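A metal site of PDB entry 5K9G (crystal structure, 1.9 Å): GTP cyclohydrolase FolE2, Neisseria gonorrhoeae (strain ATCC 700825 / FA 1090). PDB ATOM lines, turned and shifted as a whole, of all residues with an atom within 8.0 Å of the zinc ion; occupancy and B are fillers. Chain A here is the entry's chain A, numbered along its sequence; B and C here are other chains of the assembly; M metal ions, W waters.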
ATOM      1  N   LEU A 146     -29.911 -11.028 -22.237  1.00  0.00           N
ATOM      2  CA  LEU A 146     -29.364 -12.169 -21.458  1.00  0.00           C
ATOM      3  C   LEU A 146     -30.420 -13.265 -21.398  1.00  0.00           C
ATOM      4  O   LEU A 146     -31.592 -13.003 -21.086  1.00  0.00           O
ATOM      5  CB  LEU A 146     -28.855 -11.735 -20.080  1.00  0.00           C
ATOM      6  CG  LEU A 146     -28.149 -12.849 -19.247  1.00  0.00           C
ATOM      7  CD1 LEU A 146     -26.954 -12.345 -18.439  1.00  0.00           C
ATOM      8  CD2 LEU A 146     -29.189 -13.511 -18.350  1.00  0.00           C
ATOM      9  N   CYS A 147     -29.994 -14.480 -21.723  1.00  0.00           N
ATOM     10  CA  CYS A 147     -30.955 -15.523 -21.994  1.00  0.00           C
ATOM     11  C   CYS A 147     -31.490 -16.213 -20.697  1.00  0.00           C
ATOM     12  O   CYS A 147     -30.672 -16.794 -19.915  1.00  0.00           O
ATOM     13  CB  CYS A 147     -30.343 -16.560 -22.950  1.00  0.00           C
ATOM     14  SG  CYS A 147     -31.472 -17.947 -23.267  1.00  0.00           S
ATOM     15  N   PRO A 148     -32.834 -16.172 -20.457  1.00  0.00           N
ATOM     16  CA  PRO A 148     -33.414 -16.826 -19.235  1.00  0.00           C
ATOM     17  C   PRO A 148     -33.234 -18.353 -19.261  1.00  0.00           C
ATOM     18  O   PRO A 148     -32.903 -18.948 -18.231  1.00  0.00           O
ATOM     19  CB  PRO A 148     -34.908 -16.436 -19.248  1.00  0.00           C
ATOM     20  CG  PRO A 148     -35.150 -15.693 -20.536  1.00  0.00           C
ATOM     21  CD  PRO A 148     -33.880 -15.626 -21.365  1.00  0.00           C
ATOM     22  N   SNC A 149     -33.372 -18.971 -20.444  1.00  0.00           N
ATOM     23  CA  SNC A 149     -33.163 -20.417 -20.597  1.00  0.00           C
ATOM     24  CB  SNC A 149     -33.529 -20.885 -22.024  1.00  0.00           C
ATOM     25  SG  SNC A 149     -33.228 -22.636 -22.214  1.00  0.00           S
ATOM     26  ND  SNC A 149     -34.439 -23.316 -21.346  1.00  0.00           N
ATOM     27  OE  SNC A 149     -34.409 -23.382 -20.110  1.00  0.00           O
ATOM     28  C   SNC A 149     -31.763 -20.838 -20.104  1.00  0.00           C
ATOM     29  O   SNC A 149     -31.649 -21.748 -19.253  1.00  0.00           O
ATOM     30  N   SER A 150     -30.684 -20.184 -20.610  1.00  0.00           N
ATOM     31  CA  SER A 150     -29.266 -20.373 -20.223  1.00  0.00           C
ATOM     32  C   SER A 150     -29.061 -20.403 -18.690  1.00  0.00           C
ATOM     33  O   SER A 150     -28.481 -21.359 -18.135  1.00  0.00           O
ATOM     34  CB  SER A 150     -28.388 -19.254 -20.839  1.00  0.00           C
ATOM     35  OG  SER A 150     -27.002 -19.445 -20.542  1.00  0.00           O
ATOM     36  N   LYS A 151     -29.538 -19.339 -18.030  1.00  0.00           N
ATOM     37  CA  LYS A 151     -29.406 -19.156 -16.585  1.00  0.00           C
ATOM     38  C   LYS A 151     -30.107 -20.287 -15.780  1.00  0.00           C
ATOM     39  O   LYS A 151     -29.490 -20.907 -14.895  1.00  0.00           O
ATOM     40  CB  LYS A 151     -29.994 -17.794 -16.208  1.00  0.00           C
ATOM     41  CG  LYS A 151     -30.015 -17.524 -14.703  1.00  0.00           C
ATOM     42  CD  LYS A 151     -30.718 -16.203 -14.459  1.00  0.00           C
ATOM     43  CE  LYS A 151     -31.074 -16.078 -12.992  1.00  0.00           C
ATOM     44  NZ  LYS A 151     -31.311 -14.654 -12.665  1.00  0.00           N
ATOM     45  N   ILE A 153     -31.170 -23.320 -16.692  1.00  0.00           N
ATOM     46  CA  ILE A 153     -30.704 -24.701 -16.910  1.00  0.00           C
ATOM     47  C   ILE A 153     -29.258 -24.902 -16.440  1.00  0.00           C
ATOM     48  O   ILE A 153     -28.847 -26.059 -16.241  1.00  0.00           O
ATOM     49  CB  ILE A 153     -30.830 -25.187 -18.385  1.00  0.00           C
ATOM     50  CG1 ILE A 153     -29.815 -24.469 -19.346  1.00  0.00           C
ATOM     51  CG2 ILE A 153     -32.292 -25.200 -18.827  1.00  0.00           C
ATOM     52  CD1 ILE A 153     -29.752 -25.027 -20.753  1.00  0.00           C
ATOM     53  N   ALA A 158     -24.744 -17.408 -17.533  1.00  0.00           N
ATOM     54  CA  ALA A 158     -25.797 -17.321 -18.560  1.00  0.00           C
ATOM     55  C   ALA A 158     -25.249 -16.615 -19.773  1.00  0.00           C
ATOM     56  O   ALA A 158     -24.605 -15.545 -19.651  1.00  0.00           O
ATOM     57  CB  ALA A 158     -27.022 -16.553 -18.059  1.00  0.00           C
ATOM     58  N   HIS A 159     -25.560 -17.170 -20.939  1.00  0.00           N
ATOM     59  CA  HIS A 159     -25.066 -16.515 -22.155  1.00  0.00           C
ATOM     60  C   HIS A 159     -25.836 -15.179 -22.343  1.00  0.00           C
ATOM     61  O   HIS A 159     -27.016 -15.038 -21.931  1.00  0.00           O
ATOM     62  CB  HIS A 159     -25.031 -17.468 -23.382  1.00  0.00           C
ATOM     63  CG  HIS A 159     -26.299 -17.503 -24.181  1.00  0.00           C
ATOM     64  ND1 HIS A 159     -26.630 -16.520 -25.089  1.00  0.00           N
ATOM     65  CD2 HIS A 159     -27.305 -18.418 -24.237  1.00  0.00           C
ATOM     66  CE1 HIS A 159     -27.773 -16.817 -25.676  1.00  0.00           C
ATOM     67  NE2 HIS A 159     -28.208 -17.975 -25.181  1.00  0.00           N
ATOM     68  N   ASN A 160     -25.110 -14.207 -22.889  1.00  0.00           N
ATOM     69  CA  ASN A 160     -25.603 -12.846 -23.169  1.00  0.00           C
ATOM     70  C   ASN A 160     -24.793 -12.274 -24.357  1.00  0.00           C
ATOM     71  O   ASN A 160     -23.773 -12.860 -24.772  1.00  0.00           O
ATOM     72  CB  ASN A 160     -25.531 -11.936 -21.899  1.00  0.00           C
ATOM     73  CG  ASN A 160     -24.152 -11.944 -21.221  1.00  0.00           C
ATOM     74  OD1 ASN A 160     -23.238 -11.164 -21.586  1.00  0.00           O
ATOM     75  ND2 ASN A 160     -23.992 -12.825 -20.225  1.00  0.00           N
ATOM     76  N   GLN A 161     -25.271 -11.179 -24.923  1.00  0.00           N
ATOM     77  CA  GLN A 161     -24.768 -10.643 -26.211  1.00  0.00           C
ATOM     78  C   GLN A 161     -25.375  -9.257 -26.401  1.00  0.00           C
ATOM     79  O   GLN A 161     -26.447  -8.967 -25.843  1.00  0.00           O
ATOM     80  CB  GLN A 161     -25.201 -11.561 -27.386  1.00  0.00           C
ATOM     81  CG  GLN A 161     -26.709 -11.839 -27.486  1.00  0.00           C
ATOM     82  CD  GLN A 161     -27.161 -12.970 -26.556  1.00  0.00           C
ATOM     83  OE1 GLN A 161     -26.484 -14.017 -26.458  1.00  0.00           O
ATOM     84  NE2 GLN A 161     -28.282 -12.762 -25.840  1.00  0.00           N
ATOM     85  N   PHE A 214     -35.822 -13.085 -23.149  1.00  0.00           N
ATOM     86  CA  PHE A 214     -35.826 -13.558 -24.535  1.00  0.00           C
ATOM     87  C   PHE A 214     -36.038 -12.378 -25.505  1.00  0.00           C
ATOM     88  O   PHE A 214     -36.590 -11.320 -25.135  1.00  0.00           O
ATOM     89  CB  PHE A 214     -36.985 -14.563 -24.703  1.00  0.00           C
ATOM     90  CG  PHE A 214     -36.781 -15.908 -24.020  1.00  0.00           C
ATOM     91  CD1 PHE A 214     -35.686 -16.734 -24.336  1.00  0.00           C
ATOM     92  CD2 PHE A 214     -37.745 -16.385 -23.095  1.00  0.00           C
ATOM     93  CE1 PHE A 214     -35.524 -17.990 -23.726  1.00  0.00           C
ATOM     94  CE2 PHE A 214     -37.574 -17.637 -22.483  1.00  0.00           C
ATOM     95  CZ  PHE A 214     -36.456 -18.424 -22.792  1.00  0.00           C
ATOM     96  N   ASN A 241     -30.863 -10.463 -31.592  1.00  0.00           N
ATOM     97  CA  ASN A 241     -29.935 -10.806 -30.529  1.00  0.00           C
ATOM     98  C   ASN A 241     -28.820 -11.562 -31.161  1.00  0.00           C
ATOM     99  O   ASN A 241     -29.066 -12.636 -31.750  1.00  0.00           O
ATOM    100  CB  ASN A 241     -30.572 -11.792 -29.548  1.00  0.00           C
ATOM    101  CG  ASN A 241     -31.498 -11.153 -28.530  1.00  0.00           C
ATOM    102  OD1 ASN A 241     -31.894 -11.819 -27.574  1.00  0.00           O
ATOM    103  ND2 ASN A 241     -31.869  -9.882 -28.721  1.00  0.00           N
ATOM    104  N   GLU A 243     -26.762 -13.840 -30.761  1.00  0.00           N
ATOM    105  CA  GLU A 243     -26.565 -15.008 -29.884  1.00  0.00           C
ATOM    106  C   GLU A 243     -25.104 -15.365 -29.750  1.00  0.00           C
ATOM    107  O   GLU A 243     -24.442 -15.641 -30.795  1.00  0.00           O
ATOM    108  CB  GLU A 243     -27.278 -16.236 -30.457  1.00  0.00           C
ATOM    109  CG  GLU A 243     -28.784 -16.112 -30.430  1.00  0.00           C
ATOM    110  CD  GLU A 243     -29.317 -16.233 -29.013  1.00  0.00           C
ATOM    111  OE1 GLU A 243     -29.402 -17.381 -28.503  1.00  0.00           O
ATOM    112  OE2 GLU A 243     -29.617 -15.175 -28.410  1.00  0.00           O
ATOM    113  N   SER A 244     -24.628 -15.339 -28.504  1.00  0.00           N
ATOM    114  CA  SER A 244     -23.180 -15.505 -28.258  1.00  0.00           C
ATOM    115  C   SER A 244     -22.753 -16.978 -28.409  1.00  0.00           C
ATOM    116  O   SER A 244     -21.548 -17.254 -28.453  1.00  0.00           O
ATOM    117  CB  SER A 244     -22.794 -14.971 -26.867  1.00  0.00           C
ATOM    118  OG  SER A 244     -23.489 -15.727 -25.858  1.00  0.00           O
ATOM    119  N   ILE A 245     -23.744 -17.879 -28.502  1.00  0.00           N
ATOM    120  CA  ILE A 245     -23.560 -19.347 -28.612  1.00  0.00           C
ATOM    121  C   ILE A 245     -23.740 -19.926 -30.042  1.00  0.00           C
ATOM    122  O   ILE A 245     -23.411 -21.094 -30.299  1.00  0.00           O
ATOM    123  CB  ILE A 245     -24.461 -20.087 -27.587  1.00  0.00           C
ATOM    124  CG1 ILE A 245     -25.959 -19.910 -27.886  1.00  0.00           C
ATOM    125  CG2 ILE A 245     -24.113 -19.632 -26.156  1.00  0.00           C
ATOM    126  CD1 ILE A 245     -26.853 -20.883 -27.144  1.00  0.00           C
ATOM    127  N   HIS A 246     -24.262 -19.090 -30.949  1.00  0.00           N
ATOM    128  CA  HIS A 246     -24.545 -19.440 -32.364  1.00  0.00           C
ATOM    129  C   HIS A 246     -23.797 -18.517 -33.277  1.00  0.00           C
ATOM    130  O   HIS A 246     -23.216 -17.521 -32.810  1.00  0.00           O
ATOM    131  CB  HIS A 246     -26.016 -19.241 -32.673  1.00  0.00           C
ATOM    132  CG  HIS A 246     -26.918 -20.127 -31.874  1.00  0.00           C
ATOM    133  ND1 HIS A 246     -26.746 -21.500 -31.813  1.00  0.00           N
ATOM    134  CD2 HIS A 246     -28.025 -19.855 -31.130  1.00  0.00           C
ATOM    135  CE1 HIS A 246     -27.690 -22.029 -31.051  1.00  0.00           C
ATOM    136  NE2 HIS A 246     -28.499 -21.062 -30.647  1.00  0.00           N
ATOM    137  N   ALA A 250     -31.095 -14.570 -33.093  1.00  0.00           N
ATOM    138  CA  ALA A 250     -32.505 -14.724 -32.732  1.00  0.00           C
ATOM    139  C   ALA A 250     -33.202 -13.432 -33.076  1.00  0.00           C
ATOM    140  O   ALA A 250     -32.665 -12.331 -32.861  1.00  0.00           O
ATOM    141  CB  ALA A 250     -32.627 -15.065 -31.220  1.00  0.00           C
ATOM    142  N   LEU B 196     -28.198 -26.440 -31.152  1.00  0.00           N
ATOM    143  CA  LEU B 196     -27.944 -26.765 -29.763  1.00  0.00           C
ATOM    144  C   LEU B 196     -29.275 -27.163 -29.120  1.00  0.00           C
ATOM    145  O   LEU B 196     -30.256 -26.421 -29.246  1.00  0.00           O
ATOM    146  CB  LEU B 196     -27.240 -25.600 -29.043  1.00  0.00           C
ATOM    147  CG  LEU B 196     -25.755 -25.330 -29.437  1.00  0.00           C
ATOM    148  CD1 LEU B 196     -25.268 -23.962 -28.905  1.00  0.00           C
ATOM    149  CD2 LEU B 196     -24.783 -26.488 -29.074  1.00  0.00           C
ATOM    150  N   GLU B 201     -26.807 -26.548 -24.676  1.00  0.00           N
ATOM    151  CA  GLU B 201     -26.823 -25.162 -24.178  1.00  0.00           C
ATOM    152  C   GLU B 201     -26.353 -25.069 -22.686  1.00  0.00           C
ATOM    153  O   GLU B 201     -25.569 -24.120 -22.324  1.00  0.00           O
ATOM    154  CB  GLU B 201     -28.177 -24.460 -24.420  1.00  0.00           C
ATOM    155  CG  GLU B 201     -28.168 -23.037 -23.839  1.00  0.00           C
ATOM    156  CD  GLU B 201     -29.347 -22.164 -24.237  1.00  0.00           C
ATOM    157  OE1 GLU B 201     -30.435 -22.675 -24.595  1.00  0.00           O
ATOM    158  OE2 GLU B 201     -29.147 -20.931 -24.150  1.00  0.00           O
ATOM    159  N   VAL B 204     -22.465 -25.578 -23.025  1.00  0.00           N
ATOM    160  CA  VAL B 204     -21.704 -24.414 -23.541  1.00  0.00           C
ATOM    161  C   VAL B 204     -21.701 -23.213 -22.522  1.00  0.00           C
ATOM    162  O   VAL B 204     -20.613 -22.593 -22.249  1.00  0.00           O
ATOM    163  CB  VAL B 204     -22.108 -23.997 -25.010  1.00  0.00           C
ATOM    164  CG1 VAL B 204     -21.976 -25.177 -26.001  1.00  0.00           C
ATOM    165  CG2 VAL B 204     -23.505 -23.350 -25.082  1.00  0.00           C
ATOM    166  N   THR B 205     -22.878 -22.951 -21.917  1.00  0.00           N
ATOM    167  CA  THR B 205     -23.031 -21.914 -20.857  1.00  0.00           C
ATOM    168  C   THR B 205     -21.957 -22.116 -19.758  1.00  0.00           C
ATOM    169  O   THR B 205     -21.192 -21.190 -19.406  1.00  0.00           O
ATOM    170  CB  THR B 205     -24.490 -21.812 -20.282  1.00  0.00           C
ATOM    171  OG1 THR B 205     -25.402 -21.402 -21.327  1.00  0.00           O
ATOM    172  CG2 THR B 205     -24.602 -20.805 -19.102  1.00  0.00           C
ATOM    173  N   MET C  60     -36.312 -22.310 -31.038  1.00  0.00           N
ATOM    174  CA  MET C  60     -35.322 -21.777 -31.960  1.00  0.00           C
ATOM    175  C   MET C  60     -34.477 -22.839 -32.652  1.00  0.00           C
ATOM    176  O   MET C  60     -34.173 -22.708 -33.850  1.00  0.00           O
ATOM    177  CB  MET C  60     -34.395 -20.832 -31.156  1.00  0.00           C
ATOM    178  CG  MET C  60     -35.085 -19.549 -30.688  1.00  0.00           C
ATOM    179  SD  MET C  60     -35.267 -18.440 -32.122  1.00  0.00           S
ATOM    180  CE  MET C  60     -35.972 -16.955 -31.406  1.00  0.00           C
HETATM  181 ZN    ZN M   1     -30.180 -19.151 -24.949  1.00  0.00          ZN
HETATM  182  O   HOH W   1     -32.408 -20.431 -25.288  1.00  0.00           O
HETATM  183  O   HOH W   2     -30.826 -19.625 -27.483  1.00  0.00           O
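The side-chain hydroxyl of Thr 205 of chain B sits at hydrogen-bond distance from the backbone carbonyl oxygen of Glu 201 of chain B, at 2.9 Å.
The backbone NH (N) of His 159 lies within hydrogen-bond range of the side-chain hydroxyl (OG) of Ser 150 (2.7 Å).
A ring nitrogen (ND1) of His 159 lies within hydrogen-bond range of the side-chain amide oxygen (OE1) of Gln 161 (2.9 Å).
ND1 of His 159 lies within hydrogen-bond range of OG of Ser 244, 3.3 Å away.
SG of Cys 147 lies close to N of Ser 150 (3.6 Å).
The side-chain sulfur (SG) of Cys 147 lies close to N of SNC 149.
The zinc ion is bound by the side-chain carboxylate (OE2) of Glu 201 of chain B (2.2 Å), a ring nitrogen (NE2) of His 159 (2.3 Å), the side-chain sulfur (SG) of Cys 147 (2.4 Å) and water W1 (2.6 Å).
The zinc ion has four donor atoms within binding distance.
Slightly farther from the zinc ion lies water W2 (2.7 Å).
Of the 23 residues printed, 3 come within 4 Å of the zinc ion.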
